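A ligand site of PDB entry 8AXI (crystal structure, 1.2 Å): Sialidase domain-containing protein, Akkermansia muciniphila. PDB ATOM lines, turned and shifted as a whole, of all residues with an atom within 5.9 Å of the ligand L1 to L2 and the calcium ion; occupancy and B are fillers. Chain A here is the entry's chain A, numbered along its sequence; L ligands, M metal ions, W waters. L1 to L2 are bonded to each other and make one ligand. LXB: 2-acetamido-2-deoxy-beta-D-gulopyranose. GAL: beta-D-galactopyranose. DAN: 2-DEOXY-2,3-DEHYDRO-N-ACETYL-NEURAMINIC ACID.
The calcium ion is bound by the side-chain carboxylate (OE2) of Glu 278, 2.3 Å away. Water W2 is bound to the calcium ion, 2.3 Å away. The calcium ion is bound by OE1 of Glu 268. The calcium ion is bound by water W4 (2.4 Å). OD1 of Asp 279 is bound to the calcium ion, at 2.4 Å. Water W6 binds the calcium ion. The calcium ion is bound by OE2 of Glu 268, 2.6 Å away. The calcium ion has seven donor atoms within binding distance.
Water W4 bridges OE1 of Glu 278 (2.7 Å) and N of Trp 191 (3.1 Å). Water W6 lies within hydrogen-bond range of O of Val 189 (2.7 Å), O of Ala 272 (3.2 Å) and N of Trp 191 (3.3 Å). Water W3 lies within hydrogen-bond range of an oxygen (O6) of GAL L2, the backbone carbonyl oxygen of Glu 278 and the side-chain sulfur of Cys 391. Water W7 lies within hydrogen-bond range of an oxygen (O4) of DAN L3 (2.7 Å) and an oxygen (O2) of GAL L2 (3.0 Å).
The backbone carbonyl oxygen (O) of Glu 278 lies within hydrogen-bond range of the side-chain sulfur (SG) of Cys 391, at 3.6 Å. OE2 of Glu 278 sits close to N of Val 280 (3.3 Å). ND1 of His 390 is in hydrogen-bond range of OD2 of Asp 324 (2.9 Å). The side-chain amino group (NZ) of Lys 69 is in salt-bridge range of the side-chain carboxylate (OD1) of Asp 324 (3.9 Å). O of Thr 276 is in hydrogen-bond range of NE1 of Trp 191 (2.9 Å). The backbone carbonyl oxygen (O) of Cys 391 lies within hydrogen-bond range of the backbone NH (N) of Phe 281 (2.9 Å).
CH2 of Trp 191 touches C5 of GAL L2 (3.7 Å). Trp 277 touches the ligand L1 to L2. Phe 281 touches the ligand L1 to L2. Cys 391 touches the ligand L1 to L2. Hydrophobic or aromatic side chains within 4 Å of the ligand L1 to L2: Trp 191, Trp 277, Phe 281 and His 390. Seven residues have an atom within 4 Å of the ligand L1 to L2: Trp 191, Trp 277, Glu 278, Phe 281, Asp 324, His 390 and Cys 391. Along chain A the residues within 4 Å of the ligand L1 to L2 span positions 191 to 391.
Three residues have an atom within 4 Å of the calcium ion: Glu 268, Glu 278 and Asp 279. The nearest printed residue that does not touch the calcium ion is Val 280 (4.2 Å).
An oxygen (O6) of GAL L2 lies within hydrogen-bond range of the backbone NH (N) of Glu 278 (3.0 Å). OD1 of Asp 324 lies within hydrogen-bond range of O3 of GAL L2, 2.7 Å away. An oxygen (O4) of LXB L1 is in hydrogen-bond range of a ring nitrogen (NE2) of His 390 (2.9 Å). An oxygen (O1A) of DAN L3 is in salt-bridge range of the guanidinium group (NH1) of Arg 284, 2.8 Å away. An oxygen (O1A) of DAN L3 is in hydrogen-bond range of the side-chain amide nitrogen (NE2) of Gln 346, at 3.2 Å.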
ATOM      1  N   LYS A  69      37.949  -9.212  10.768  1.00  0.00           N
ATOM      2  CA  LYS A  69      37.034  -9.194   9.620  1.00  0.00           C
ATOM      3  C   LYS A  69      35.801  -8.319   9.824  1.00  0.00           C
ATOM      4  O   LYS A  69      34.965  -8.241   8.928  1.00  0.00           O
ATOM      5  CB  LYS A  69      36.614 -10.614   9.248  1.00  0.00           C
ATOM      6  CG  LYS A  69      35.635 -11.238  10.211  1.00  0.00           C
ATOM      7  CD  LYS A  69      35.527 -12.738   9.924  1.00  0.00           C
ATOM      8  CE  LYS A  69      34.477 -13.369  10.760  1.00  0.00           C
ATOM      9  NZ  LYS A  69      34.339 -14.821  10.390  1.00  0.00           N
ATOM     10  N   VAL A 189      19.847 -32.148  14.511  1.00  0.00           N
ATOM     11  CA  VAL A 189      19.397 -30.850  15.032  1.00  0.00           C
ATOM     12  C   VAL A 189      20.216 -29.737  14.414  1.00  0.00           C
ATOM     13  O   VAL A 189      21.423 -29.879  14.175  1.00  0.00           O
ATOM     14  CB  VAL A 189      19.457 -30.792  16.573  1.00  0.00           C
ATOM     15  CG1 VAL A 189      18.494 -31.791  17.198  1.00  0.00           C
ATOM     16  CG2 VAL A 189      20.875 -31.019  17.064  1.00  0.00           C
ATOM     17  N   ARG A 190      19.559 -28.618  14.170  1.00  0.00           N
ATOM     18  CA  ARG A 190      20.241 -27.416  13.745  1.00  0.00           C
ATOM     19  C   ARG A 190      21.084 -26.843  14.879  1.00  0.00           C
ATOM     20  O   ARG A 190      20.758 -26.978  16.065  1.00  0.00           O
ATOM     21  CB  ARG A 190      19.227 -26.361  13.334  1.00  0.00           C
ATOM     22  CG  ARG A 190      18.480 -26.713  12.068  1.00  0.00           C
ATOM     23  CD  ARG A 190      17.580 -25.546  11.671  1.00  0.00           C
ATOM     24  NE  ARG A 190      16.843 -25.784  10.426  1.00  0.00           N
ATOM     25  CZ  ARG A 190      15.642 -25.291  10.166  1.00  0.00           C
ATOM     26  NH1 ARG A 190      14.973 -24.572  11.063  1.00  0.00           N
ATOM     27  NH2 ARG A 190      15.073 -25.546   8.979  1.00  0.00           N
ATOM     28  N   TRP A 191      22.166 -26.165  14.510  1.00  0.00           N
ATOM     29  CA  TRP A 191      22.922 -25.350  15.441  1.00  0.00           C
ATOM     30  C   TRP A 191      21.971 -24.450  16.211  1.00  0.00           C
ATOM     31  O   TRP A 191      21.169 -23.741  15.613  1.00  0.00           O
ATOM     32  CB  TRP A 191      23.844 -24.464  14.598  1.00  0.00           C
ATOM     33  CG  TRP A 191      24.791 -23.546  15.354  1.00  0.00           C
ATOM     34  CD1 TRP A 191      25.268 -23.704  16.625  1.00  0.00           C
ATOM     35  CD2 TRP A 191      25.396 -22.357  14.826  1.00  0.00           C
ATOM     36  NE1 TRP A 191      26.116 -22.656  16.922  1.00  0.00           N
ATOM     37  CE2 TRP A 191      26.230 -21.828  15.839  1.00  0.00           C
ATOM     38  CE3 TRP A 191      25.341 -21.711  13.591  1.00  0.00           C
ATOM     39  CZ2 TRP A 191      26.978 -20.674  15.653  1.00  0.00           C
ATOM     40  CZ3 TRP A 191      26.072 -20.545  13.417  1.00  0.00           C
ATOM     41  CH2 TRP A 191      26.891 -20.041  14.442  1.00  0.00           C
ATOM     42  N   LEU A 243      19.450 -18.828  11.148  1.00  0.00           N
ATOM     43  CA  LEU A 243      20.884 -18.735  11.459  1.00  0.00           C
ATOM     44  C   LEU A 243      21.566 -17.735  10.531  1.00  0.00           C
ATOM     45  O   LEU A 243      22.718 -17.918  10.131  1.00  0.00           O
ATOM     46  CB  LEU A 243      21.587 -20.111  11.478  1.00  0.00           C
ATOM     47  CG  LEU A 243      21.023 -21.086  12.544  1.00  0.00           C
ATOM     48  CD1 LEU A 243      21.453 -22.512  12.235  1.00  0.00           C
ATOM     49  CD2 LEU A 243      21.464 -20.671  13.969  1.00  0.00           C
ATOM     50  N   GLU A 268      18.667 -31.128   7.995  1.00  0.00           N
ATOM     51  CA  GLU A 268      19.841 -31.627   8.683  1.00  0.00           C
ATOM     52  C   GLU A 268      20.104 -33.087   8.315  1.00  0.00           C
ATOM     53  O   GLU A 268      19.181 -33.881   8.145  1.00  0.00           O
ATOM     54  CB  GLU A 268      19.591 -31.518  10.180  1.00  0.00           C
ATOM     55  CG  GLU A 268      19.721 -30.158  10.876  1.00  0.00           C
ATOM     56  CD  GLU A 268      20.876 -29.334  10.365  1.00  0.00           C
ATOM     57  OE1 GLU A 268      22.031 -29.818  10.521  1.00  0.00           O
ATOM     58  OE2 GLU A 268      20.727 -28.112  10.080  1.00  0.00           O
ATOM     59  N   ALA A 272      24.861 -34.277  11.861  1.00  0.00           N
ATOM     60  CA  ALA A 272      24.733 -32.824  12.045  1.00  0.00           C
ATOM     61  C   ALA A 272      25.369 -32.321  13.335  1.00  0.00           C
ATOM     62  O   ALA A 272      25.559 -31.098  13.462  1.00  0.00           O
ATOM     63  CB  ALA A 272      23.268 -32.387  11.969  1.00  0.00           C
ATOM     64  N   THR A 276      25.653 -27.565  19.383  1.00  0.00           N
ATOM     65  CA  THR A 276      26.492 -26.509  19.968  1.00  0.00           C
ATOM     66  C   THR A 276      27.043 -25.590  18.886  1.00  0.00           C
ATOM     67  O   THR A 276      27.009 -24.356  19.029  1.00  0.00           O
ATOM     68  CB  THR A 276      27.640 -27.115  20.762  1.00  0.00           C
ATOM     69  OG1 THR A 276      27.131 -28.003  21.763  1.00  0.00           O
ATOM     70  CG2 THR A 276      28.472 -26.012  21.421  1.00  0.00           C
ATOM     71  N   TRP A 277      27.572 -26.163  17.811  1.00  0.00           N
ATOM     72  CA  TRP A 277      28.094 -25.420  16.681  1.00  0.00           C
ATOM     73  C   TRP A 277      27.486 -25.966  15.392  1.00  0.00           C
ATOM     74  O   TRP A 277      26.756 -26.962  15.395  1.00  0.00           O
ATOM     75  CB  TRP A 277      29.639 -25.457  16.631  1.00  0.00           C
ATOM     76  CG  TRP A 277      30.330 -24.745  17.790  1.00  0.00           C
ATOM     77  CD1 TRP A 277      30.995 -25.338  18.830  1.00  0.00           C
ATOM     78  CD2 TRP A 277      30.457 -23.330  17.993  1.00  0.00           C
ATOM     79  NE1 TRP A 277      31.507 -24.372  19.675  1.00  0.00           N
ATOM     80  CE2 TRP A 277      31.199 -23.139  19.182  1.00  0.00           C
ATOM     81  CE3 TRP A 277      30.019 -22.209  17.282  1.00  0.00           C
ATOM     82  CZ2 TRP A 277      31.486 -21.865  19.689  1.00  0.00           C
ATOM     83  CZ3 TRP A 277      30.308 -20.943  17.784  1.00  0.00           C
ATOM     84  CH2 TRP A 277      31.047 -20.787  18.968  1.00  0.00           C
ATOM     85  N   GLU A 278      27.754 -25.262  14.302  1.00  0.00           N
ATOM     86  CA  GLU A 278      27.231 -25.647  12.997  1.00  0.00           C
ATOM     87  C   GLU A 278      28.026 -26.790  12.382  1.00  0.00           C
ATOM     88  O   GLU A 278      29.222 -26.969  12.658  1.00  0.00           O
ATOM     89  CB  GLU A 278      27.331 -24.427  12.085  1.00  0.00           C
ATOM     90  CG  GLU A 278      26.709 -24.629  10.712  1.00  0.00           C
ATOM     91  CD  GLU A 278      25.260 -25.087  10.808  1.00  0.00           C
ATOM     92  OE1 GLU A 278      24.359 -24.213  10.956  1.00  0.00           O
ATOM     93  OE2 GLU A 278      25.020 -26.319  10.727  1.00  0.00           O
ATOM     94  N   ASP A 279      27.337 -27.632  11.591  1.00  0.00           N
ATOM     95  CA  ASP A 279      28.069 -28.591  10.757  1.00  0.00           C
ATOM     96  C   ASP A 279      28.378 -28.028   9.382  1.00  0.00           C
ATOM     97  O   ASP A 279      29.523 -28.109   8.904  1.00  0.00           O
ATOM     98  CB  ASP A 279      27.399 -29.988  10.713  1.00  0.00           C
ATOM     99  CG  ASP A 279      26.065 -30.020   9.962  1.00  0.00           C
ATOM    100  OD1 ASP A 279      25.235 -29.112  10.126  1.00  0.00           O
ATOM    101  OD2 ASP A 279      25.804 -31.035   9.275  1.00  0.00           O
ATOM    102  N   VAL A 280      27.383 -27.463   8.711  1.00  0.00           N
ATOM    103  CA  VAL A 280      27.572 -26.964   7.360  1.00  0.00           C
ATOM    104  C   VAL A 280      26.500 -25.914   7.058  1.00  0.00           C
ATOM    105  O   VAL A 280      25.343 -26.064   7.448  1.00  0.00           O
ATOM    106  CB  VAL A 280      27.550 -28.118   6.325  1.00  0.00           C
ATOM    107  CG1 VAL A 280      26.163 -28.812   6.283  1.00  0.00           C
ATOM    108  CG2 VAL A 280      27.967 -27.595   4.963  1.00  0.00           C
ATOM    109  N   PHE A 281      26.896 -24.869   6.358  1.00  0.00           N
ATOM    110  CA  PHE A 281      25.966 -23.827   5.930  1.00  0.00           C
ATOM    111  C   PHE A 281      25.453 -24.122   4.520  1.00  0.00           C
ATOM    112  O   PHE A 281      26.240 -24.245   3.574  1.00  0.00           O
ATOM    113  CB  PHE A 281      26.688 -22.480   5.924  1.00  0.00           C
ATOM    114  CG  PHE A 281      27.021 -21.975   7.299  1.00  0.00           C
ATOM    115  CD1 PHE A 281      26.003 -21.696   8.194  1.00  0.00           C
ATOM    116  CD2 PHE A 281      28.338 -21.838   7.695  1.00  0.00           C
ATOM    117  CE1 PHE A 281      26.300 -21.221   9.472  1.00  0.00           C
ATOM    118  CE2 PHE A 281      28.643 -21.365   8.979  1.00  0.00           C
ATOM    119  CZ  PHE A 281      27.602 -21.081   9.856  1.00  0.00           C
ATOM    120  N   ARG A 284      23.236 -19.524   2.682  1.00  0.00           N
ATOM    121  CA  ARG A 284      23.812 -18.182   2.820  1.00  0.00           C
ATOM    122  C   ARG A 284      24.212 -17.552   1.496  1.00  0.00           C
ATOM    123  O   ARG A 284      25.086 -16.693   1.462  1.00  0.00           O
ATOM    124  CB  ARG A 284      24.993 -18.152   3.795  1.00  0.00           C
ATOM    125  CG  ARG A 284      24.579 -18.412   5.232  1.00  0.00           C
ATOM    126  CD  ARG A 284      25.754 -18.410   6.173  1.00  0.00           C
ATOM    127  NE  ARG A 284      25.301 -18.415   7.568  1.00  0.00           N
ATOM    128  CZ  ARG A 284      26.052 -18.004   8.573  1.00  0.00           C
ATOM    129  NH1 ARG A 284      27.310 -17.649   8.380  1.00  0.00           N
ATOM    130  NH2 ARG A 284      25.537 -17.976   9.806  1.00  0.00           N
ATOM    131  N   ASP A 324      34.298 -17.494   6.961  1.00  0.00           N
ATOM    132  CA  ASP A 324      32.884 -17.454   6.629  1.00  0.00           C
ATOM    133  C   ASP A 324      32.634 -16.623   5.389  1.00  0.00           C
ATOM    134  O   ASP A 324      33.179 -15.528   5.221  1.00  0.00           O
ATOM    135  CB  ASP A 324      32.098 -16.860   7.801  1.00  0.00           C
ATOM    136  CG  ASP A 324      31.970 -17.836   8.962  1.00  0.00           C
ATOM    137  OD1 ASP A 324      31.444 -17.423  10.017  1.00  0.00           O
ATOM    138  OD2 ASP A 324      32.381 -19.000   8.807  1.00  0.00           O
ATOM    139  N   GLN A 346      29.904 -11.662   3.535  1.00  0.00           N
ATOM    140  CA  GLN A 346      31.089 -11.993   4.311  1.00  0.00           C
ATOM    141  C   GLN A 346      32.120 -12.568   3.359  1.00  0.00           C
ATOM    142  O   GLN A 346      31.774 -13.299   2.428  1.00  0.00           O
ATOM    143  CB  GLN A 346      30.795 -13.085   5.335  1.00  0.00           C
ATOM    144  CG  GLN A 346      29.790 -12.695   6.401  1.00  0.00           C
ATOM    145  CD  GLN A 346      29.423 -13.890   7.254  1.00  0.00           C
ATOM    146  OE1 GLN A 346      28.984 -14.924   6.734  1.00  0.00           O
ATOM    147  NE2 GLN A 346      29.620 -13.798   8.552  1.00  0.00           N
ATOM    148  N   HIS A 390      35.558 -24.157   6.499  1.00  0.00           N
ATOM    149  CA  HIS A 390      34.880 -23.950   7.767  1.00  0.00           C
ATOM    150  C   HIS A 390      33.369 -24.081   7.532  1.00  0.00           C
ATOM    151  O   HIS A 390      32.752 -23.197   6.959  1.00  0.00           O
ATOM    152  CB  HIS A 390      35.242 -22.605   8.366  1.00  0.00           C
ATOM    153  CG  HIS A 390      34.559 -22.331   9.661  1.00  0.00           C
ATOM    154  ND1 HIS A 390      33.515 -21.445   9.784  1.00  0.00           N
ATOM    155  CD2 HIS A 390      34.731 -22.875  10.888  1.00  0.00           C
ATOM    156  CE1 HIS A 390      33.093 -21.432  11.041  1.00  0.00           C
ATOM    157  NE2 HIS A 390      33.807 -22.292  11.730  1.00  0.00           N
ATOM    158  N   CYS A 391      32.810 -25.225   7.926  1.00  0.00           N
ATOM    159  CA  CYS A 391      31.373 -25.480   7.810  1.00  0.00           C
ATOM    160  C   CYS A 391      30.837 -25.223   6.409  1.00  0.00           C
ATOM    161  O   CYS A 391      29.755 -24.663   6.246  1.00  0.00           O
ATOM    162  CB  CYS A 391      30.572 -24.660   8.832  1.00  0.00           C
ATOM    163  SG  CYS A 391      31.147 -24.745  10.523  1.00  0.00           S
HETATM  164  O1  LXB L   1      36.783 -22.029  18.119  1.00  0.00           O
HETATM  165  C1  LXB L   1      35.568 -22.117  17.446  1.00  0.00           C
HETATM  166  C2  LXB L   1      35.633 -21.253  16.183  1.00  0.00           C
HETATM  167  C3  LXB L   1      34.398 -21.421  15.292  1.00  0.00           C
HETATM  168  C4  LXB L   1      33.833 -22.850  15.249  1.00  0.00           C
HETATM  169  C5  LXB L   1      33.986 -23.628  16.550  1.00  0.00           C
HETATM  170  C6  LXB L   1      33.784 -25.111  16.360  1.00  0.00           C
HETATM  171  C7  LXB L   1      36.810 -19.104  16.247  1.00  0.00           C
HETATM  172  C8  LXB L   1      36.793 -17.698  16.778  1.00  0.00           C
HETATM  173  N2  LXB L   1      35.768 -19.865  16.572  1.00  0.00           N
HETATM  174  O3  LXB L   1      33.436 -20.439  15.708  1.00  0.00           O
HETATM  175  O4  LXB L   1      34.535 -23.559  14.224  1.00  0.00           O
HETATM  176  O5  LXB L   1      35.312 -23.467  17.096  1.00  0.00           O
HETATM  177  O6  LXB L   1      34.089 -25.855  17.535  1.00  0.00           O
HETATM  178  O7  LXB L   1      37.722 -19.521  15.539  1.00  0.00           O
HETATM  179  C1  GAL L   2      32.353 -20.075  14.874  1.00  0.00           C
HETATM  180  C2  GAL L   2      32.571 -18.853  13.991  1.00  0.00           C
HETATM  181  C3  GAL L   2      31.201 -18.367  13.545  1.00  0.00           C
HETATM  182  C4  GAL L   2      30.423 -19.477  12.846  1.00  0.00           C
HETATM  183  C5  GAL L   2      30.443 -20.757  13.697  1.00  0.00           C
HETATM  184  C6  GAL L   2      29.830 -21.978  13.048  1.00  0.00           C
HETATM  185  O2  GAL L   2      33.252 -17.835  14.726  1.00  0.00           O
HETATM  186  O3  GAL L   2      31.304 -17.204  12.714  1.00  0.00           O
HETATM  187  O4  GAL L   2      30.956 -19.744  11.550  1.00  0.00           O
HETATM  188  O5  GAL L   2      31.795 -21.109  14.053  1.00  0.00           O
HETATM  189  O6  GAL L   2      29.731 -23.030  14.009  1.00  0.00           O
HETATM  190  C1  DAN L   3      28.194 -16.351  11.691  1.00  0.00           C
HETATM  191  C2  DAN L   3      28.791 -15.443  12.780  1.00  0.00           C
HETATM  192  C3  DAN L   3      29.805 -14.241  12.387  1.00  0.00           C
HETATM  193  C4  DAN L   3      30.170 -13.474  13.490  1.00  0.00           C
HETATM  194  C5  DAN L   3      29.935 -14.338  14.879  1.00  0.00           C
HETATM  195  C6  DAN L   3      28.610 -14.568  15.097  1.00  0.00           C
HETATM  196  C7  DAN L   3      28.288 -15.512  16.256  1.00  0.00           C
HETATM  197  C8  DAN L   3      26.792 -15.816  16.205  1.00  0.00           C
HETATM  198  C9  DAN L   3      26.393 -16.822  17.313  1.00  0.00           C
HETATM  199  C10 DAN L   3      31.408 -14.088  17.046  1.00  0.00           C
HETATM  200  C11 DAN L   3      32.010 -13.175  18.129  1.00  0.00           C
HETATM  201  N5  DAN L   3      30.537 -13.476  15.964  1.00  0.00           N
HETATM  202  O1A DAN L   3      28.405 -16.052  10.437  1.00  0.00           O
HETATM  203  O1B DAN L   3      27.538 -17.316  12.219  1.00  0.00           O
HETATM  204  O4  DAN L   3      31.566 -13.085  13.343  1.00  0.00           O
HETATM  205  O6  DAN L   3      27.933 -15.279  13.835  1.00  0.00           O
HETATM  206  O7  DAN L   3      29.000 -16.696  16.133  1.00  0.00           O
HETATM  207  O8  DAN L   3      26.076 -14.644  16.380  1.00  0.00           O
HETATM  208  O9  DAN L   3      26.811 -16.333  18.585  1.00  0.00           O
HETATM  209  O10 DAN L   3      31.610 -15.294  17.041  1.00  0.00           O
HETATM  210 CA    CA M   1      23.291 -27.849  10.589  1.00  0.00          CA
HETATM  211  O   HOH W   1      37.148 -23.369  13.637  1.00  0.00           O
HETATM  212  O   HOH W   2      23.121 -27.220   8.343  1.00  0.00           O
HETATM  213  O   HOH W   3      31.566 -25.287  13.738  1.00  0.00           O
HETATM  214  O   HOH W   4      22.247 -25.893  11.408  1.00  0.00           O
HETATM  215  O   HOH W   5      35.265 -14.644  16.021  1.00  0.00           O
HETATM  216  O   HOH W   6      23.478 -28.686  12.833  1.00  0.00           O
HETATM  217  O   HOH W   7      33.351 -14.867  14.204  1.00  0.00           O
